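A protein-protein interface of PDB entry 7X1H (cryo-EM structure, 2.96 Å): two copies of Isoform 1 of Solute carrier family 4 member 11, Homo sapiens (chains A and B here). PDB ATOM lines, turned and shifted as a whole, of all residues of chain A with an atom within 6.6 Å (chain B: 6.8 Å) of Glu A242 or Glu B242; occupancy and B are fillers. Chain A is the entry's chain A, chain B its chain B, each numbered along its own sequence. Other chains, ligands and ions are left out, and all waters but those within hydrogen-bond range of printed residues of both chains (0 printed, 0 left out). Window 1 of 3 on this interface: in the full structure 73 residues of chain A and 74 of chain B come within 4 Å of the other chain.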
ATOM      1  N   ARG A 112     -13.391  -4.795 -41.398  1.00  0.00           N
ATOM      2  CA  ARG A 112     -12.330  -3.903 -40.951  1.00  0.00           C
ATOM      3  C   ARG A 112     -11.225  -3.862 -41.995  1.00  0.00           C
ATOM      4  O   ARG A 112     -10.870  -4.889 -42.580  1.00  0.00           O
ATOM      5  CB  ARG A 112     -11.764  -4.358 -39.604  1.00  0.00           C
ATOM      6  CG  ARG A 112     -12.501  -3.787 -38.403  1.00  0.00           C
ATOM      7  CD  ARG A 112     -12.705  -4.830 -37.316  1.00  0.00           C
ATOM      8  NE  ARG A 112     -13.661  -4.384 -36.309  1.00  0.00           N
ATOM      9  CZ  ARG A 112     -14.444  -5.188 -35.603  1.00  0.00           C
ATOM     10  NH1 ARG A 112     -14.406  -6.503 -35.753  1.00  0.00           N
ATOM     11  NH2 ARG A 112     -15.286  -4.661 -34.719  1.00  0.00           N
ATOM     12  N   VAL A 208      -5.578  -3.276 -28.299  1.00  0.00           N
ATOM     13  CA  VAL A 208      -5.885  -2.342 -29.375  1.00  0.00           C
ATOM     14  C   VAL A 208      -6.601  -1.147 -28.758  1.00  0.00           C
ATOM     15  O   VAL A 208      -7.724  -1.271 -28.263  1.00  0.00           O
ATOM     16  CB  VAL A 208      -6.734  -3.002 -30.467  1.00  0.00           C
ATOM     17  CG1 VAL A 208      -7.314  -1.951 -31.399  1.00  0.00           C
ATOM     18  CG2 VAL A 208      -5.905  -4.013 -31.245  1.00  0.00           C
ATOM     19  N   TYR A 210      -8.339   2.399 -29.259  1.00  0.00           N
ATOM     20  CA  TYR A 210      -8.987   3.256 -30.238  1.00  0.00           C
ATOM     21  C   TYR A 210      -8.916   4.712 -29.798  1.00  0.00           C
ATOM     22  O   TYR A 210      -8.936   5.024 -28.605  1.00  0.00           O
ATOM     23  CB  TYR A 210     -10.450   2.850 -30.429  1.00  0.00           C
ATOM     24  CG  TYR A 210     -10.650   1.631 -31.299  1.00  0.00           C
ATOM     25  CD1 TYR A 210     -10.450   0.353 -30.794  1.00  0.00           C
ATOM     26  CD2 TYR A 210     -11.042   1.755 -32.623  1.00  0.00           C
ATOM     27  CE1 TYR A 210     -10.634  -0.764 -31.584  1.00  0.00           C
ATOM     28  CE2 TYR A 210     -11.228   0.645 -33.421  1.00  0.00           C
ATOM     29  CZ  TYR A 210     -11.023  -0.612 -32.897  1.00  0.00           C
ATOM     30  OH  TYR A 210     -11.208  -1.721 -33.688  1.00  0.00           O
ATOM     31  N   GLN A 212     -10.907   7.448 -29.221  1.00  0.00           N
ATOM     32  CA  GLN A 212     -12.331   7.634 -28.985  1.00  0.00           C
ATOM     33  C   GLN A 212     -12.744   9.099 -28.951  1.00  0.00           C
ATOM     34  O   GLN A 212     -13.929   9.387 -28.758  1.00  0.00           O
ATOM     35  CB  GLN A 212     -12.734   6.959 -27.670  1.00  0.00           C
ATOM     36  CG  GLN A 212     -12.005   5.652 -27.399  1.00  0.00           C
ATOM     37  CD  GLN A 212     -12.569   4.905 -26.210  1.00  0.00           C
ATOM     38  OE1 GLN A 212     -13.413   5.420 -25.480  1.00  0.00           O
ATOM     39  NE2 GLN A 212     -12.103   3.677 -26.009  1.00  0.00           N
ATOM     40  N   ASN A 239     -20.991   9.306 -25.709  1.00  0.00           N
ATOM     41  CA  ASN A 239     -20.694   7.906 -26.058  1.00  0.00           C
ATOM     42  C   ASN A 239     -21.316   7.462 -27.367  1.00  0.00           C
ATOM     43  O   ASN A 239     -22.415   6.947 -27.376  1.00  0.00           O
ATOM     44  CB  ASN A 239     -21.216   7.002 -24.937  1.00  0.00           C
ATOM     45  CG  ASN A 239     -20.819   5.540 -25.086  1.00  0.00           C
ATOM     46  OD1 ASN A 239     -20.309   5.109 -26.111  1.00  0.00           O
ATOM     47  ND2 ASN A 239     -21.071   4.765 -24.043  1.00  0.00           N
ATOM     48  N   TRP A 240     -20.592   7.575 -28.468  1.00  0.00           N
ATOM     49  CA  TRP A 240     -21.172   7.253 -29.765  1.00  0.00           C
ATOM     50  C   TRP A 240     -21.056   5.797 -30.196  1.00  0.00           C
ATOM     51  O   TRP A 240     -21.513   5.435 -31.275  1.00  0.00           O
ATOM     52  CB  TRP A 240     -20.608   8.178 -30.835  1.00  0.00           C
ATOM     53  CG  TRP A 240     -21.318   9.465 -30.920  1.00  0.00           C
ATOM     54  CD1 TRP A 240     -21.617  10.305 -29.895  1.00  0.00           C
ATOM     55  CD2 TRP A 240     -21.829  10.072 -32.102  1.00  0.00           C
ATOM     56  NE1 TRP A 240     -22.290  11.401 -30.364  1.00  0.00           N
ATOM     57  CE2 TRP A 240     -22.432  11.281 -31.720  1.00  0.00           C
ATOM     58  CE3 TRP A 240     -21.839   9.710 -33.449  1.00  0.00           C
ATOM     59  CZ2 TRP A 240     -23.036  12.128 -32.634  1.00  0.00           C
ATOM     60  CZ3 TRP A 240     -22.442  10.550 -34.352  1.00  0.00           C
ATOM     61  CH2 TRP A 240     -23.032  11.745 -33.944  1.00  0.00           C
ATOM     62  N   GLY A 241     -20.437   4.964 -29.377  1.00  0.00           N
ATOM     63  CA  GLY A 241     -20.278   3.570 -29.730  1.00  0.00           C
ATOM     64  C   GLY A 241     -19.403   2.773 -28.791  1.00  0.00           C
ATOM     65  O   GLY A 241     -18.988   3.272 -27.758  1.00  0.00           O
ATOM     66  N   GLU A 242     -19.113   1.527 -29.143  1.00  0.00           N
ATOM     67  CA  GLU A 242     -18.317   0.663 -28.276  1.00  0.00           C
ATOM     68  C   GLU A 242     -16.895   1.141 -28.053  1.00  0.00           C
ATOM     69  O   GLU A 242     -16.383   1.086 -26.938  1.00  0.00           O
ATOM     70  CB  GLU A 242     -18.275  -0.744 -28.864  1.00  0.00           C
ATOM     71  CG  GLU A 242     -17.699  -1.791 -27.932  1.00  0.00           C
ATOM     72  CD  GLU A 242     -18.521  -1.954 -26.670  1.00  0.00           C
ATOM     73  OE1 GLU A 242     -19.692  -2.374 -26.774  1.00  0.00           O
ATOM     74  OE2 GLU A 242     -17.995  -1.669 -25.574  1.00  0.00           O
ATOM     75  N   ASN A 243     -16.243   1.595 -29.111  1.00  0.00           N
ATOM     76  CA  ASN A 243     -14.878   2.081 -29.000  1.00  0.00           C
ATOM     77  C   ASN A 243     -14.859   3.567 -29.239  1.00  0.00           C
ATOM     78  O   ASN A 243     -13.823   4.129 -29.561  1.00  0.00           O
ATOM     79  CB  ASN A 243     -13.983   1.345 -29.976  1.00  0.00           C
ATOM     80  CG  ASN A 243     -13.704  -0.076 -29.540  1.00  0.00           C
ATOM     81  OD1 ASN A 243     -13.308  -0.317 -28.402  1.00  0.00           O
ATOM     82  ND2 ASN A 243     -13.902  -1.026 -30.446  1.00  0.00           N
ATOM     83  N   SER A 244     -16.021   4.195 -29.139  1.00  0.00           N
ATOM     84  CA  SER A 244     -16.126   5.625 -29.336  1.00  0.00           C
ATOM     85  C   SER A 244     -16.887   6.169 -28.158  1.00  0.00           C
ATOM     86  O   SER A 244     -17.845   6.904 -28.333  1.00  0.00           O
ATOM     87  CB  SER A 244     -16.897   5.898 -30.613  1.00  0.00           C
ATOM     88  OG  SER A 244     -16.217   5.384 -31.738  1.00  0.00           O
ATOM     89  N   CYS A 245     -16.465   5.830 -26.949  1.00  0.00           N
ATOM     90  CA  CYS A 245     -17.217   6.221 -25.764  1.00  0.00           C
ATOM     91  C   CYS A 245     -17.046   7.687 -25.387  1.00  0.00           C
ATOM     92  O   CYS A 245     -17.817   8.183 -24.559  1.00  0.00           O
ATOM     93  CB  CYS A 245     -16.802   5.343 -24.581  1.00  0.00           C
ATOM     94  SG  CYS A 245     -16.949   3.567 -24.889  1.00  0.00           S
ATOM     95  N   VAL A 739     -12.234   4.909 -22.454  1.00  0.00           N
ATOM     96  CA  VAL A 739     -13.007   3.911 -21.724  1.00  0.00           C
ATOM     97  C   VAL A 739     -12.599   2.543 -22.257  1.00  0.00           C
ATOM     98  O   VAL A 739     -13.010   2.141 -23.351  1.00  0.00           O
ATOM     99  CB  VAL A 739     -14.516   4.140 -21.862  1.00  0.00           C
ATOM    100  CG1 VAL A 739     -15.286   3.084 -21.086  1.00  0.00           C
ATOM    101  CG2 VAL A 739     -14.887   5.535 -21.383  1.00  0.00           C
ATOM    102  N   GLU A 740     -11.788   1.824 -21.485  1.00  0.00           N
ATOM    103  CA  GLU A 740     -11.396   0.455 -21.797  1.00  0.00           C
ATOM    104  C   GLU A 740     -11.907  -0.452 -20.689  1.00  0.00           C
ATOM    105  O   GLU A 740     -11.559  -0.263 -19.518  1.00  0.00           O
ATOM    106  CB  GLU A 740      -9.878   0.330 -21.939  1.00  0.00           C
ATOM    107  CG  GLU A 740      -9.294   1.083 -23.123  1.00  0.00           C
ATOM    108  CD  GLU A 740      -9.731   0.511 -24.457  1.00  0.00           C
ATOM    109  OE1 GLU A 740      -9.950  -0.716 -24.537  1.00  0.00           O
ATOM    110  OE2 GLU A 740      -9.856   1.288 -25.427  1.00  0.00           O
ATOM    111  N   ASN A 741     -12.726  -1.441 -21.042  1.00  0.00           N
ATOM    112  CA  ASN A 741     -13.303  -2.373 -20.058  1.00  0.00           C
ATOM    113  C   ASN A 741     -14.100  -1.650 -18.993  1.00  0.00           C
ATOM    114  O   ASN A 741     -14.101  -2.040 -17.830  1.00  0.00           O
ATOM    115  CB  ASN A 741     -12.249  -3.293 -19.433  1.00  0.00           C
ATOM    116  CG  ASN A 741     -12.846  -4.587 -18.910  1.00  0.00           C
ATOM    117  OD1 ASN A 741     -12.611  -4.976 -17.768  1.00  0.00           O
ATOM    118  ND2 ASN A 741     -13.640  -5.250 -19.742  1.00  0.00           N
ATOM    119  N   PRO A 817      -7.888  -9.819 -26.645  1.00  0.00           N
ATOM    120  CA  PRO A 817      -7.167 -10.646 -27.619  1.00  0.00           C
ATOM    121  C   PRO A 817      -5.692 -10.313 -27.822  1.00  0.00           C
ATOM    122  O   PRO A 817      -4.884 -11.236 -27.879  1.00  0.00           O
ATOM    123  CB  PRO A 817      -7.943 -10.396 -28.916  1.00  0.00           C
ATOM    124  CG  PRO A 817      -8.952  -9.333 -28.621  1.00  0.00           C
ATOM    125  CD  PRO A 817      -9.196  -9.395 -27.153  1.00  0.00           C
ATOM    126  N   ARG B 112     -20.410  -1.883 -41.346  1.00  0.00           N
ATOM    127  CA  ARG B 112     -21.445  -2.730 -40.772  1.00  0.00           C
ATOM    128  C   ARG B 112     -22.600  -2.860 -41.754  1.00  0.00           C
ATOM    129  O   ARG B 112     -22.983  -1.886 -42.411  1.00  0.00           O
ATOM    130  CB  ARG B 112     -21.946  -2.158 -39.445  1.00  0.00           C
ATOM    131  CG  ARG B 112     -21.153  -2.627 -38.236  1.00  0.00           C
ATOM    132  CD  ARG B 112     -20.897  -1.496 -37.255  1.00  0.00           C
ATOM    133  NE  ARG B 112     -19.893  -1.856 -36.260  1.00  0.00           N
ATOM    134  CZ  ARG B 112     -19.077  -0.995 -35.665  1.00  0.00           C
ATOM    135  NH1 ARG B 112     -19.123   0.301 -35.927  1.00  0.00           N
ATOM    136  NH2 ARG B 112     -18.192  -1.448 -34.781  1.00  0.00           N
ATOM    137  N   VAL B 208     -27.593  -2.230 -27.799  1.00  0.00           N
ATOM    138  CA  VAL B 208     -27.329  -3.258 -28.799  1.00  0.00           C
ATOM    139  C   VAL B 208     -26.584  -4.393 -28.107  1.00  0.00           C
ATOM    140  O   VAL B 208     -25.445  -4.222 -27.666  1.00  0.00           O
ATOM    141  CB  VAL B 208     -26.529  -2.699 -29.982  1.00  0.00           C
ATOM    142  CG1 VAL B 208     -26.004  -3.829 -30.849  1.00  0.00           C
ATOM    143  CG2 VAL B 208     -27.390  -1.749 -30.800  1.00  0.00           C
ATOM    144  N   TYR B 210     -24.857  -7.973 -28.393  1.00  0.00           N
ATOM    145  CA  TYR B 210     -24.256  -8.911 -29.325  1.00  0.00           C
ATOM    146  C   TYR B 210     -24.293 -10.322 -28.755  1.00  0.00           C
ATOM    147  O   TYR B 210     -24.209 -10.527 -27.541  1.00  0.00           O
ATOM    148  CB  TYR B 210     -22.809  -8.522 -29.629  1.00  0.00           C
ATOM    149  CG  TYR B 210     -22.664  -7.396 -30.627  1.00  0.00           C
ATOM    150  CD1 TYR B 210     -22.871  -6.077 -30.250  1.00  0.00           C
ATOM    151  CD2 TYR B 210     -22.317  -7.653 -31.946  1.00  0.00           C
ATOM    152  CE1 TYR B 210     -22.736  -5.045 -31.161  1.00  0.00           C
ATOM    153  CE2 TYR B 210     -22.181  -6.629 -32.862  1.00  0.00           C
ATOM    154  CZ  TYR B 210     -22.392  -5.329 -32.465  1.00  0.00           C
ATOM    155  OH  TYR B 210     -22.259  -4.304 -33.373  1.00  0.00           O
ATOM    156  N   GLN B 212     -22.263 -12.999 -28.031  1.00  0.00           N
ATOM    157  CA  GLN B 212     -20.829 -13.220 -27.850  1.00  0.00           C
ATOM    158  C   GLN B 212     -20.397 -14.656 -27.752  1.00  0.00           C
ATOM    159  O   GLN B 212     -19.219 -14.926 -27.637  1.00  0.00           O
ATOM    160  CB  GLN B 212     -20.419 -12.537 -26.556  1.00  0.00           C
ATOM    161  CG  GLN B 212     -21.235 -11.301 -26.228  1.00  0.00           C
ATOM    162  CD  GLN B 212     -20.582 -10.436 -25.176  1.00  0.00           C
ATOM    163  OE1 GLN B 212     -19.854 -10.930 -24.323  1.00  0.00           O
ATOM    164  NE2 GLN B 212     -20.848  -9.138 -25.227  1.00  0.00           N
ATOM    165  N   ASN B 239     -11.938 -14.360 -24.942  1.00  0.00           N
ATOM    166  CA  ASN B 239     -12.198 -12.994 -25.408  1.00  0.00           C
ATOM    167  C   ASN B 239     -11.617 -12.805 -26.796  1.00  0.00           C
ATOM    168  O   ASN B 239     -10.406 -12.761 -26.956  1.00  0.00           O
ATOM    169  CB  ASN B 239     -11.578 -11.995 -24.438  1.00  0.00           C
ATOM    170  CG  ASN B 239     -12.042 -10.575 -24.666  1.00  0.00           C
ATOM    171  OD1 ASN B 239     -12.748 -10.289 -25.620  1.00  0.00           O
ATOM    172  ND2 ASN B 239     -11.643  -9.676 -23.780  1.00  0.00           N
ATOM    173  N   TRP B 240     -12.467 -12.671 -27.806  1.00  0.00           N
ATOM    174  CA  TRP B 240     -11.983 -12.581 -29.170  1.00  0.00           C
ATOM    175  C   TRP B 240     -12.251 -11.205 -29.736  1.00  0.00           C
ATOM    176  O   TRP B 240     -12.127 -10.991 -30.937  1.00  0.00           O
ATOM    177  CB  TRP B 240     -12.644 -13.652 -30.031  1.00  0.00           C
ATOM    178  CG  TRP B 240     -11.957 -14.967 -29.998  1.00  0.00           C
ATOM    179  CD1 TRP B 240     -11.641 -15.700 -28.898  1.00  0.00           C
ATOM    180  CD2 TRP B 240     -11.508 -15.718 -31.125  1.00  0.00           C
ATOM    181  NE1 TRP B 240     -11.010 -16.858 -29.267  1.00  0.00           N
ATOM    182  CE2 TRP B 240     -10.917 -16.893 -30.632  1.00  0.00           C
ATOM    183  CE3 TRP B 240     -11.542 -15.508 -32.504  1.00  0.00           C
ATOM    184  CZ2 TRP B 240     -10.365 -17.853 -31.468  1.00  0.00           C
ATOM    185  CZ3 TRP B 240     -10.992 -16.459 -33.329  1.00  0.00           C
ATOM    186  CH2 TRP B 240     -10.413 -17.618 -32.812  1.00  0.00           C
ATOM    187  N   GLY B 241     -12.614 -10.268 -28.874  1.00  0.00           N
ATOM    188  CA  GLY B 241     -12.877  -8.919 -29.326  1.00  0.00           C
ATOM    189  C   GLY B 241     -13.769  -8.151 -28.380  1.00  0.00           C
ATOM    190  O   GLY B 241     -14.119  -8.661 -27.328  1.00  0.00           O
ATOM    191  N   GLU B 242     -14.155  -6.932 -28.745  1.00  0.00           N
ATOM    192  CA  GLU B 242     -14.952  -6.105 -27.844  1.00  0.00           C
ATOM    193  C   GLU B 242     -16.334  -6.658 -27.566  1.00  0.00           C
ATOM    194  O   GLU B 242     -16.810  -6.608 -26.435  1.00  0.00           O
ATOM    195  CB  GLU B 242     -15.080  -4.676 -28.368  1.00  0.00           C
ATOM    196  CG  GLU B 242     -14.077  -3.701 -27.775  1.00  0.00           C
ATOM    197  CD  GLU B 242     -14.480  -3.200 -26.400  1.00  0.00           C
ATOM    198  OE1 GLU B 242     -15.618  -3.477 -25.966  1.00  0.00           O
ATOM    199  OE2 GLU B 242     -13.657  -2.517 -25.753  1.00  0.00           O
ATOM    200  N   ASN B 243     -16.998  -7.156 -28.596  1.00  0.00           N
ATOM    201  CA  ASN B 243     -18.305  -7.746 -28.399  1.00  0.00           C
ATOM    202  C   ASN B 243     -18.235  -9.252 -28.466  1.00  0.00           C
ATOM    203  O   ASN B 243     -19.208  -9.916 -28.169  1.00  0.00           O
ATOM    204  CB  ASN B 243     -19.275  -7.183 -29.421  1.00  0.00           C
ATOM    205  CG  ASN B 243     -19.528  -5.704 -29.216  1.00  0.00           C
ATOM    206  OD1 ASN B 243     -19.854  -5.267 -28.114  1.00  0.00           O
ATOM    207  ND2 ASN B 243     -19.387  -4.925 -30.281  1.00  0.00           N
ATOM    208  N   SER B 244     -17.070  -9.812 -28.757  1.00  0.00           N
ATOM    209  CA  SER B 244     -16.919 -11.260 -28.767  1.00  0.00           C
ATOM    210  C   SER B 244     -16.198 -11.723 -27.522  1.00  0.00           C
ATOM    211  O   SER B 244     -15.262 -12.503 -27.608  1.00  0.00           O
ATOM    212  CB  SER B 244     -16.153 -11.682 -30.008  1.00  0.00           C
ATOM    213  OG  SER B 244     -16.742 -11.143 -31.173  1.00  0.00           O
ATOM    214  N   CYS B 245     -16.641 -11.276 -26.358  1.00  0.00           N
ATOM    215  CA  CYS B 245     -15.943 -11.592 -25.114  1.00  0.00           C
ATOM    216  C   CYS B 245     -16.039 -13.007 -24.545  1.00  0.00           C
ATOM    217  O   CYS B 245     -15.223 -13.378 -23.708  1.00  0.00           O
ATOM    218  CB  CYS B 245     -16.349 -10.603 -24.032  1.00  0.00           C
ATOM    219  SG  CYS B 245     -15.929  -8.886 -24.381  1.00  0.00           S
ATOM    220  N   VAL B 739     -20.613  -9.914 -21.600  1.00  0.00           N
ATOM    221  CA  VAL B 739     -19.807  -8.859 -20.997  1.00  0.00           C
ATOM    222  C   VAL B 739     -20.241  -7.542 -21.627  1.00  0.00           C
ATOM    223  O   VAL B 739     -19.886  -7.236 -22.771  1.00  0.00           O
ATOM    224  CB  VAL B 739     -18.305  -9.104 -21.191  1.00  0.00           C
ATOM    225  CG1 VAL B 739     -17.499  -7.989 -20.546  1.00  0.00           C
ATOM    226  CG2 VAL B 739     -17.911 -10.456 -20.615  1.00  0.00           C
ATOM    227  N   GLU B 740     -21.015  -6.756 -20.881  1.00  0.00           N
ATOM    228  CA  GLU B 740     -21.423  -5.418 -21.291  1.00  0.00           C
ATOM    229  C   GLU B 740     -20.859  -4.419 -20.293  1.00  0.00           C
ATOM    230  O   GLU B 740     -21.149  -4.504 -19.094  1.00  0.00           O
ATOM    231  CB  GLU B 740     -22.947  -5.301 -21.366  1.00  0.00           C
ATOM    232  CG  GLU B 740     -23.589  -6.153 -22.450  1.00  0.00           C
ATOM    233  CD  GLU B 740     -23.218  -5.700 -23.849  1.00  0.00           C
ATOM    234  OE1 GLU B 740     -23.007  -4.485 -24.046  1.00  0.00           O
ATOM    235  OE2 GLU B 740     -23.141  -6.559 -24.753  1.00  0.00           O
ATOM    236  N   ASN B 741     -20.060  -3.475 -20.786  1.00  0.00           N
ATOM    237  CA  ASN B 741     -19.443  -2.452 -19.942  1.00  0.00           C
ATOM    238  C   ASN B 741     -18.610  -3.083 -18.827  1.00  0.00           C
ATOM    239  O   ASN B 741     -18.584  -2.595 -17.695  1.00  0.00           O
ATOM    240  CB  ASN B 741     -20.500  -1.513 -19.361  1.00  0.00           C
ATOM    241  CG  ASN B 741     -19.924  -0.177 -18.937  1.00  0.00           C
ATOM    242  OD1 ASN B 741     -19.973   0.190 -17.764  1.00  0.00           O
ATOM    243  ND2 ASN B 741     -19.374   0.560 -19.895  1.00  0.00           N
ATOM    244  N   PRO B 817     -25.181   4.312 -27.055  1.00  0.00           N
ATOM    245  CA  PRO B 817     -26.020   5.180 -27.891  1.00  0.00           C
ATOM    246  C   PRO B 817     -27.482   4.805 -27.946  1.00  0.00           C
ATOM    247  O   PRO B 817     -28.327   5.694 -28.010  1.00  0.00           O
ATOM    248  CB  PRO B 817     -25.424   5.005 -29.282  1.00  0.00           C
ATOM    249  CG  PRO B 817     -24.053   4.511 -29.070  1.00  0.00           C
ATOM    250  CD  PRO B 817     -24.160   3.628 -27.882  1.00  0.00           C
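Asn A239 touches Pro B817, and with the chains exchanged Pro A817 touches Asn B239.
Trp A240 touches Pro B817, and with the chains exchanged Pro A817 touches Trp B240.
Gly A241 touches Pro B817, and with the chains exchanged Pro A817 touches Gly B241.
Glu A242 touches Asn B243, and with the chains exchanged Asn A243 touches Glu B242.
15 positions are printed for both chains.
Printed residues of chain B within 4 Å of Trp A240: Pro B817 (3.5 Å).
Glu A242 touches just these residues of chain B: Glu B242 (3.0 Å) and Asn B243 (3.2 Å).
Printed residues of chain A within 4 Å of Asn B243: Glu A242.
The nearest printed residue of chain B that does not touch Gly A241 is Arg B112 (7.1 Å).
Among the printed residues, merely in contact across the chains: Asn A239 with Pro B817, Trp A240 with Pro B817, Pro A817 with Asn B239, Gly A241 with Pro B817, Pro A817 with Gly B241 and Pro A817 with Trp B240.
Of the 15 printed residues of chain A, 6 touch a printed residue of chain B.
Printed residues of chain A that touch a printed residue of chain B: Asn A239, Trp A240, Gly A241, Glu A242, Asn A243 and Pro A817.
Hydrophobic or aromatic side chains of chain A that line the printed part of chain B: Pro A817.
Along chain A the printed residues that touch a printed residue of chain B span positions 239 to 817.
Of the 15 printed residues of chain B, 6 touch a printed residue of chain A.
Printed residues of chain B that touch a printed residue of chain A: Asn B239, Trp B240, Gly B241, Glu B242, Asn B243 and Pro B817.
Hydrophobic or aromatic side chains of chain B within 4 Å of the printed part of chain A: Pro B817.
The side-chain amide nitrogen of Gln B212 lies close to the backbone carbonyl oxygen of Asn B243, at 3.5 Å.
O of Gly A241 sits at hydrogen-bond distance from SG of Cys A245 (3.5 Å).
OD1 of Asn B239 lies close to O of Gly B241.
The side-chain amide oxygen of Asn A239 lies close to the backbone carbonyl oxygen of Gly A241 (2.8 Å).
SG of Cys B245 is in hydrogen-bond range of O of Gly B241, 3.5 Å away.
OD1 of Asn B239 sits close to SG of Cys B245, at 3.7 Å.
OE2 of Glu A242 lies close to OE1 of Glu B242 (3.0 Å).
The side-chain carboxylate of Glu B242 lies close to the side-chain amide oxygen of Asn A243.
OD1 of Asn B243 lies close to OE1 of Glu A242 (3.2 Å).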
